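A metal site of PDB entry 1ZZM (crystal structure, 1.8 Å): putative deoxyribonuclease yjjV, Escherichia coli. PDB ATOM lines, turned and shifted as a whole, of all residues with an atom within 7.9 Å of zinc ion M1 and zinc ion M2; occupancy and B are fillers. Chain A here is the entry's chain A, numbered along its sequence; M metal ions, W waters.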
ATOM      1  N   HIS A   9     -19.667   6.714  -5.949  1.00  0.00           N
ATOM      2  CA  HIS A   9     -19.376   7.259  -7.279  1.00  0.00           C
ATOM      3  C   HIS A   9     -19.077   8.762  -7.162  1.00  0.00           C
ATOM      4  O   HIS A   9     -19.985   9.578  -7.145  1.00  0.00           O
ATOM      5  CB  HIS A   9     -20.617   7.051  -8.174  1.00  0.00           C
ATOM      6  CG  HIS A   9     -20.348   7.246  -9.638  1.00  0.00           C
ATOM      7  ND1 HIS A   9     -20.224   6.194 -10.515  1.00  0.00           N
ATOM      8  CD2 HIS A   9     -20.203   8.372 -10.365  1.00  0.00           C
ATOM      9  CE1 HIS A   9     -20.013   6.678 -11.738  1.00  0.00           C
ATOM     10  NE2 HIS A   9     -19.990   7.994 -11.661  1.00  0.00           N
ATOM     11  N   CYS A  10     -17.809   9.106  -7.037  1.00  0.00           N
ATOM     12  CA  CYS A  10     -17.436  10.502  -6.958  1.00  0.00           C
ATOM     13  C   CYS A  10     -16.180  10.716  -7.791  1.00  0.00           C
ATOM     14  O   CYS A  10     -15.168  10.030  -7.600  1.00  0.00           O
ATOM     15  CB  CYS A  10     -17.162  10.899  -5.491  1.00  0.00           C
ATOM     16  SG  CYS A  10     -16.589  12.655  -5.332  1.00  0.00           S
ATOM     17  N   HIS A  11     -16.238  11.671  -8.733  1.00  0.00           N
ATOM     18  CA  HIS A  11     -15.103  11.966  -9.600  1.00  0.00           C
ATOM     19  C   HIS A  11     -14.191  12.910  -8.824  1.00  0.00           C
ATOM     20  O   HIS A  11     -14.029  14.088  -9.163  1.00  0.00           O
ATOM     21  CB  HIS A  11     -15.613  12.601 -10.900  1.00  0.00           C
ATOM     22  CG  HIS A  11     -16.368  11.639 -11.757  1.00  0.00           C
ATOM     23  ND1 HIS A  11     -15.743  10.690 -12.528  1.00  0.00           N
ATOM     24  CD2 HIS A  11     -17.702  11.397 -11.877  1.00  0.00           C
ATOM     25  CE1 HIS A  11     -16.640   9.892 -13.075  1.00  0.00           C
ATOM     26  NE2 HIS A  11     -17.843  10.297 -12.690  1.00  0.00           N
ATOM     27  N   PRO A  39     -14.283   6.523  -9.855  1.00  0.00           N
ATOM     28  CA  PRO A  39     -14.168   5.834 -11.143  1.00  0.00           C
ATOM     29  C   PRO A  39     -13.447   6.703 -12.169  1.00  0.00           C
ATOM     30  O   PRO A  39     -13.730   7.913 -12.271  1.00  0.00           O
ATOM     31  CB  PRO A  39     -15.609   5.550 -11.508  1.00  0.00           C
ATOM     32  CG  PRO A  39     -16.372   6.677 -10.901  1.00  0.00           C
ATOM     33  CD  PRO A  39     -15.613   7.135  -9.678  1.00  0.00           C
ATOM     34  N   ALA A  40     -12.512   6.130 -12.920  1.00  0.00           N
ATOM     35  CA  ALA A  40     -11.787   6.945 -13.912  1.00  0.00           C
ATOM     36  C   ALA A  40     -12.666   7.185 -15.127  1.00  0.00           C
ATOM     37  O   ALA A  40     -13.710   6.535 -15.293  1.00  0.00           O
ATOM     38  CB  ALA A  40     -10.523   6.276 -14.332  1.00  0.00           C
ATOM     39  N   THR A  41     -12.236   8.121 -15.985  1.00  0.00           N
ATOM     40  CA  THR A  41     -12.964   8.477 -17.209  1.00  0.00           C
ATOM     41  C   THR A  41     -12.192   8.188 -18.478  1.00  0.00           C
ATOM     42  O   THR A  41     -12.776   8.045 -19.564  1.00  0.00           O
ATOM     43  CB  THR A  41     -13.298   9.975 -17.223  1.00  0.00           C
ATOM     44  OG1 THR A  41     -12.083  10.728 -17.049  1.00  0.00           O
ATOM     45  CG2 THR A  41     -14.309  10.312 -16.057  1.00  0.00           C
ATOM     46  N   HIS A  66     -14.859   6.059 -19.994  1.00  0.00           N
ATOM     47  CA  HIS A  66     -16.194   6.666 -19.986  1.00  0.00           C
ATOM     48  C   HIS A  66     -16.712   6.988 -21.383  1.00  0.00           C
ATOM     49  O   HIS A  66     -15.978   7.517 -22.225  1.00  0.00           O
ATOM     50  CB  HIS A  66     -16.108   7.935 -19.102  1.00  0.00           C
ATOM     51  CG  HIS A  66     -17.436   8.457 -18.633  1.00  0.00           C
ATOM     52  ND1 HIS A  66     -18.400   8.926 -19.510  1.00  0.00           N
ATOM     53  CD2 HIS A  66     -17.907   8.709 -17.388  1.00  0.00           C
ATOM     54  CE1 HIS A  66     -19.403   9.441 -18.813  1.00  0.00           C
ATOM     55  NE2 HIS A  66     -19.123   9.329 -17.526  1.00  0.00           N
ATOM     56  N   PRO A  67     -17.991   6.668 -21.664  1.00  0.00           N
ATOM     57  CA  PRO A  67     -18.534   6.956 -23.012  1.00  0.00           C
ATOM     58  C   PRO A  67     -18.514   8.444 -23.353  1.00  0.00           C
ATOM     59  O   PRO A  67     -18.432   8.808 -24.537  1.00  0.00           O
ATOM     60  CB  PRO A  67     -19.954   6.367 -22.959  1.00  0.00           C
ATOM     61  CG  PRO A  67     -20.334   6.451 -21.490  1.00  0.00           C
ATOM     62  CD  PRO A  67     -19.021   6.070 -20.798  1.00  0.00           C
ATOM     63  N   GLU A  97     -15.972   3.300 -14.772  1.00  0.00           N
ATOM     64  CA  GLU A  97     -16.892   4.185 -15.379  1.00  0.00           C
ATOM     65  C   GLU A  97     -16.842   3.868 -16.843  1.00  0.00           C
ATOM     66  O   GLU A  97     -16.045   4.398 -17.602  1.00  0.00           O
ATOM     67  CB  GLU A  97     -16.993   5.666 -15.073  1.00  0.00           C
ATOM     68  CG  GLU A  97     -18.506   5.861 -15.426  1.00  0.00           C
ATOM     69  CD  GLU A  97     -19.199   7.120 -14.937  1.00  0.00           C
ATOM     70  OE1 GLU A  97     -18.576   8.007 -14.320  1.00  0.00           O
ATOM     71  OE2 GLU A  97     -20.422   7.191 -15.181  1.00  0.00           O
ATOM     72  N   ILE A  98     -17.684   2.899 -17.184  1.00  0.00           N
ATOM     73  CA  ILE A  98     -17.840   2.460 -18.575  1.00  0.00           C
ATOM     74  C   ILE A  98     -19.352   2.506 -18.773  1.00  0.00           C
ATOM     75  O   ILE A  98     -20.095   2.660 -17.801  1.00  0.00           O
ATOM     76  CB  ILE A  98     -17.351   1.038 -18.801  1.00  0.00           C
ATOM     77  CG1 ILE A  98     -18.227   0.042 -18.027  1.00  0.00           C
ATOM     78  CG2 ILE A  98     -15.907   0.930 -18.358  1.00  0.00           C
ATOM     79  CD1 ILE A  98     -17.696  -1.383 -18.079  1.00  0.00           C
ATOM     80  N   LEU A 100     -22.802   3.578 -21.687  1.00  0.00           N
ATOM     81  CA  LEU A 100     -23.336   4.155 -22.899  1.00  0.00           C
ATOM     82  C   LEU A 100     -24.043   5.462 -22.605  1.00  0.00           C
ATOM     83  O   LEU A 100     -24.531   5.692 -21.494  1.00  0.00           O
ATOM     84  CB  LEU A 100     -24.366   3.209 -23.516  1.00  0.00           C
ATOM     85  CG  LEU A 100     -23.884   1.759 -23.684  1.00  0.00           C
ATOM     86  CD1 LEU A 100     -25.095   0.923 -23.897  1.00  0.00           C
ATOM     87  CD2 LEU A 100     -22.860   1.623 -24.842  1.00  0.00           C
ATOM     88  N   ASP A 101     -24.133   6.331 -23.603  1.00  0.00           N
ATOM     89  CA  ASP A 101     -24.768   7.627 -23.370  1.00  0.00           C
ATOM     90  C   ASP A 101     -25.236   8.120 -24.739  1.00  0.00           C
ATOM     91  O   ASP A 101     -24.404   8.399 -25.607  1.00  0.00           O
ATOM     92  CB  ASP A 101     -23.716   8.552 -22.781  1.00  0.00           C
ATOM     93  CG  ASP A 101     -24.262   9.909 -22.373  1.00  0.00           C
ATOM     94  OD1 ASP A 101     -25.131  10.409 -23.091  1.00  0.00           O
ATOM     95  OD2 ASP A 101     -23.824  10.460 -21.335  1.00  0.00           O
ATOM     96  N   ILE A 131     -18.798  -0.439 -12.929  1.00  0.00           N
ATOM     97  CA  ILE A 131     -19.528   0.766 -12.535  1.00  0.00           C
ATOM     98  C   ILE A 131     -19.981   1.307 -13.876  1.00  0.00           C
ATOM     99  O   ILE A 131     -19.178   1.703 -14.730  1.00  0.00           O
ATOM    100  CB  ILE A 131     -18.608   1.781 -11.806  1.00  0.00           C
ATOM    101  CG1 ILE A 131     -18.364   1.279 -10.368  1.00  0.00           C
ATOM    102  CG2 ILE A 131     -19.255   3.181 -11.787  1.00  0.00           C
ATOM    103  CD1 ILE A 131     -17.417   2.223  -9.521  1.00  0.00           C
ATOM    104  N   LEU A 132     -21.290   1.317 -14.049  1.00  0.00           N
ATOM    105  CA  LEU A 132     -21.888   1.685 -15.303  1.00  0.00           C
ATOM    106  C   LEU A 132     -22.625   3.008 -15.352  1.00  0.00           C
ATOM    107  O   LEU A 132     -23.359   3.384 -14.426  1.00  0.00           O
ATOM    108  CB  LEU A 132     -22.863   0.578 -15.721  1.00  0.00           C
ATOM    109  CG  LEU A 132     -22.295  -0.824 -15.908  1.00  0.00           C
ATOM    110  CD1 LEU A 132     -23.444  -1.858 -15.772  1.00  0.00           C
ATOM    111  CD2 LEU A 132     -21.594  -0.921 -17.275  1.00  0.00           C
ATOM    112  N   HIS A 133     -22.431   3.677 -16.496  1.00  0.00           N
ATOM    113  CA  HIS A 133     -23.059   4.940 -16.846  1.00  0.00           C
ATOM    114  C   HIS A 133     -24.081   4.583 -17.914  1.00  0.00           C
ATOM    115  O   HIS A 133     -23.787   3.809 -18.844  1.00  0.00           O
ATOM    116  CB  HIS A 133     -22.021   5.887 -17.461  1.00  0.00           C
ATOM    117  CG  HIS A 133     -22.573   7.209 -17.909  1.00  0.00           C
ATOM    118  ND1 HIS A 133     -22.625   8.317 -17.099  1.00  0.00           N
ATOM    119  CD2 HIS A 133     -23.034   7.621 -19.116  1.00  0.00           C
ATOM    120  CE1 HIS A 133     -23.081   9.353 -17.772  1.00  0.00           C
ATOM    121  NE2 HIS A 133     -23.349   8.958 -19.002  1.00  0.00           N
ATOM    122  N   SER A 134     -25.292   5.127 -17.801  1.00  0.00           N
ATOM    123  CA  SER A 134     -26.334   4.855 -18.781  1.00  0.00           C
ATOM    124  C   SER A 134     -27.226   6.072 -18.865  1.00  0.00           C
ATOM    125  O   SER A 134     -27.839   6.473 -17.870  1.00  0.00           O
ATOM    126  CB  SER A 134     -27.166   3.636 -18.383  1.00  0.00           C
ATOM    127  OG  SER A 134     -28.061   3.266 -19.456  1.00  0.00           O
ATOM    128  N   ARG A 135     -27.292   6.678 -20.035  1.00  0.00           N
ATOM    129  CA  ARG A 135     -28.129   7.844 -20.164  1.00  0.00           C
ATOM    130  C   ARG A 135     -28.916   7.649 -21.461  1.00  0.00           C
ATOM    131  O   ARG A 135     -28.353   7.753 -22.574  1.00  0.00           O
ATOM    132  CB  ARG A 135     -27.247   9.078 -20.235  1.00  0.00           C
ATOM    133  CG  ARG A 135     -28.008  10.349 -20.518  1.00  0.00           C
ATOM    134  CD  ARG A 135     -27.031  11.364 -21.066  1.00  0.00           C
ATOM    135  NE  ARG A 135     -27.118  12.626 -20.370  1.00  0.00           N
ATOM    136  CZ  ARG A 135     -26.090  13.467 -20.268  1.00  0.00           C
ATOM    137  NH1 ARG A 135     -24.923  13.132 -20.820  1.00  0.00           N
ATOM    138  NH2 ARG A 135     -26.239  14.608 -19.616  1.00  0.00           N
ATOM    139  N   HIS A 157     -25.001   3.198 -12.139  1.00  0.00           N
ATOM    140  CA  HIS A 157     -24.963   4.406 -11.301  1.00  0.00           C
ATOM    141  C   HIS A 157     -25.912   5.530 -11.733  1.00  0.00           C
ATOM    142  O   HIS A 157     -26.394   5.562 -12.868  1.00  0.00           O
ATOM    143  CB  HIS A 157     -23.517   4.914 -11.251  1.00  0.00           C
ATOM    144  CG  HIS A 157     -23.288   6.174 -12.033  1.00  0.00           C
ATOM    145  ND1 HIS A 157     -23.602   7.428 -11.536  1.00  0.00           N
ATOM    146  CD2 HIS A 157     -22.846   6.366 -13.300  1.00  0.00           C
ATOM    147  CE1 HIS A 157     -23.359   8.333 -12.471  1.00  0.00           C
ATOM    148  NE2 HIS A 157     -22.897   7.722 -13.546  1.00  0.00           N
ATOM    149  N   GLY A 158     -26.194   6.428 -10.781  1.00  0.00           N
ATOM    150  CA  GLY A 158     -27.018   7.605 -11.035  1.00  0.00           C
ATOM    151  C   GLY A 158     -28.271   7.300 -11.813  1.00  0.00           C
ATOM    152  O   GLY A 158     -28.671   8.055 -12.659  1.00  0.00           O
ATOM    153  N   GLU A 205     -24.719   7.353  -3.700  1.00  0.00           N
ATOM    154  CA  GLU A 205     -23.655   8.036  -4.464  1.00  0.00           C
ATOM    155  C   GLU A 205     -24.021   9.487  -4.658  1.00  0.00           C
ATOM    156  O   GLU A 205     -25.121   9.901  -4.270  1.00  0.00           O
ATOM    157  CB  GLU A 205     -23.521   7.447  -5.865  1.00  0.00           C
ATOM    158  CG  GLU A 205     -24.738   7.790  -6.736  1.00  0.00           C
ATOM    159  CD  GLU A 205     -24.609   7.319  -8.168  1.00  0.00           C
ATOM    160  OE1 GLU A 205     -24.638   6.095  -8.393  1.00  0.00           O
ATOM    161  OE2 GLU A 205     -24.514   8.162  -9.069  1.00  0.00           O
ATOM    162  N   THR A 206     -23.098  10.245  -5.254  1.00  0.00           N
ATOM    163  CA  THR A 206     -23.367  11.646  -5.618  1.00  0.00           C
ATOM    164  C   THR A 206     -23.066  11.985  -7.091  1.00  0.00           C
ATOM    165  O   THR A 206     -23.712  12.863  -7.670  1.00  0.00           O
ATOM    166  CB  THR A 206     -22.522  12.692  -4.836  1.00  0.00           C
ATOM    167  OG1 THR A 206     -21.126  12.446  -5.068  1.00  0.00           O
ATOM    168  CG2 THR A 206     -22.854  12.674  -3.314  1.00  0.00           C
ATOM    169  N   ASP A 207     -22.089  11.292  -7.674  1.00  0.00           N
ATOM    170  CA  ASP A 207     -21.568  11.585  -9.007  1.00  0.00           C
ATOM    171  C   ASP A 207     -20.951  12.996  -8.952  1.00  0.00           C
ATOM    172  O   ASP A 207     -20.834  13.690  -9.967  1.00  0.00           O
ATOM    173  CB  ASP A 207     -22.633  11.527 -10.147  1.00  0.00           C
ATOM    174  CG  ASP A 207     -21.981  11.488 -11.555  1.00  0.00           C
ATOM    175  OD1 ASP A 207     -20.784  11.154 -11.660  1.00  0.00           O
ATOM    176  OD2 ASP A 207     -22.656  11.780 -12.559  1.00  0.00           O
ATOM    177  N   ALA A 208     -20.552  13.447  -7.764  1.00  0.00           N
ATOM    178  CA  ALA A 208     -19.943  14.787  -7.662  1.00  0.00           C
ATOM    179  C   ALA A 208     -18.705  14.856  -8.558  1.00  0.00           C
ATOM    180  O   ALA A 208     -17.938  13.900  -8.657  1.00  0.00           O
ATOM    181  CB  ALA A 208     -19.552  15.103  -6.197  1.00  0.00           C
ATOM    182  N   PRO A 209     -18.423  16.030  -9.125  1.00  0.00           N
ATOM    183  CA  PRO A 209     -19.128  17.304  -9.016  1.00  0.00           C
ATOM    184  C   PRO A 209     -20.389  17.474  -9.834  1.00  0.00           C
ATOM    185  O   PRO A 209     -21.008  18.527  -9.793  1.00  0.00           O
ATOM    186  CB  PRO A 209     -18.036  18.315  -9.393  1.00  0.00           C
ATOM    187  CG  PRO A 209     -17.402  17.616 -10.526  1.00  0.00           C
ATOM    188  CD  PRO A 209     -17.256  16.178 -10.012  1.00  0.00           C
ATOM    189  N   ASP A 210     -20.787  16.460 -10.605  1.00  0.00           N
ATOM    190  CA  ASP A 210     -22.015  16.632 -11.396  1.00  0.00           C
ATOM    191  C   ASP A 210     -23.253  16.243 -10.584  1.00  0.00           C
ATOM    192  O   ASP A 210     -23.133  15.907  -9.396  1.00  0.00           O
ATOM    193  CB  ASP A 210     -21.938  15.786 -12.680  1.00  0.00           C
ATOM    194  CG  ASP A 210     -20.747  16.182 -13.567  1.00  0.00           C
ATOM    195  OD1 ASP A 210     -20.300  17.360 -13.516  1.00  0.00           O
ATOM    196  OD2 ASP A 210     -20.263  15.316 -14.335  1.00  0.00           O
ATOM    197  N   MET A 211     -24.438  16.305 -11.215  1.00  0.00           N
ATOM    198  CA  MET A 211     -25.716  15.951 -10.579  1.00  0.00           C
ATOM    199  C   MET A 211     -25.991  16.691  -9.249  1.00  0.00           C
ATOM    200  O   MET A 211     -26.265  16.071  -8.217  1.00  0.00           O
ATOM    201  CB  MET A 211     -25.795  14.415 -10.408  1.00  0.00           C
ATOM    202  CG  MET A 211     -25.649  13.623 -11.772  1.00  0.00           C
ATOM    203  SD  MET A 211     -25.800  11.742 -11.778  1.00  0.00           S
ATOM    204  CE  MET A 211     -27.592  11.528 -11.910  1.00  0.00           C
HETATM  205 ZN    ZN M   1     -21.979   8.639 -15.189  1.00  0.00          ZN
HETATM  206 ZN    ZN M   2     -19.535   9.352 -13.180  1.00  0.00          ZN
HETATM  207  O   HOH W   1     -23.478  10.535 -15.024  1.00  0.00           O
HETATM  208  O   HOH W   2     -20.559  10.039 -14.790  1.00  0.00           O
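The nearest printed residue that does not touch zinc ion M2 is His 66 (4.4 Å).
Zinc ion M1 is bound by water W2 (2.0 Å), ND1 of His 133 (2.0 Å), NE2 of His 157 (2.1 Å), OE2 of Glu 97 (2.1 Å) and water W1 (2.4 Å).
Zinc ion M1 has five donor atoms within binding distance.
N of Leu 100 is in hydrogen-bond range of O of His 133.
A ring nitrogen (NE2) of His 133 lies within hydrogen-bond range of the side-chain carboxylate (OD2) of Asp 101, 2.8 Å away.
The backbone carbonyl oxygen (O) of His 9 lies within hydrogen-bond range of the backbone NH (N) of Asp 207 (2.8 Å).
The backbone NH of His 11 lies within hydrogen-bond range of the backbone carbonyl oxygen of Ala 208 (2.8 Å).
The backbone carbonyl oxygen (O) of Glu 97 lies within hydrogen-bond range of the backbone NH (N) of His 66.
The backbone NH (N) of His 157 sits at hydrogen-bond distance from the backbone carbonyl oxygen (O) of Leu 132, 2.8 Å away.
The side-chain carboxylate (OE2) of Glu 205 lies within hydrogen-bond range of a ring nitrogen (ND1) of His 157, 2.7 Å away.
The side-chain carboxylate (OD1) of Asp 207 lies close to a ring nitrogen (NE2) of His 11 (3.2 Å).
Merely in contact with zinc ion M1: His 66 (3.8 Å).
Along chain A the residues within 4 Å of zinc ion M1 span positions 66 to 157.
NE2 of His 11 is bound to zinc ion M2 (2.0 Å).
Zinc ion M2 is bound by the side-chain carboxylate (OE1) of Glu 97 (2.0 Å).
Water W2 binds zinc ion M2 (2.0 Å).
A ring nitrogen (NE2) of His 9 is bound to zinc ion M2 (2.1 Å).
Slightly farther from zinc ion M2 lies the side-chain carboxylate (OD1) of Asp 207 (2.7 Å).
Water W2 lies within hydrogen-bond range of a ring nitrogen (NE2) of His 66 (3.2 Å) and the side-chain carboxylate of Asp 207 (3.3 Å).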
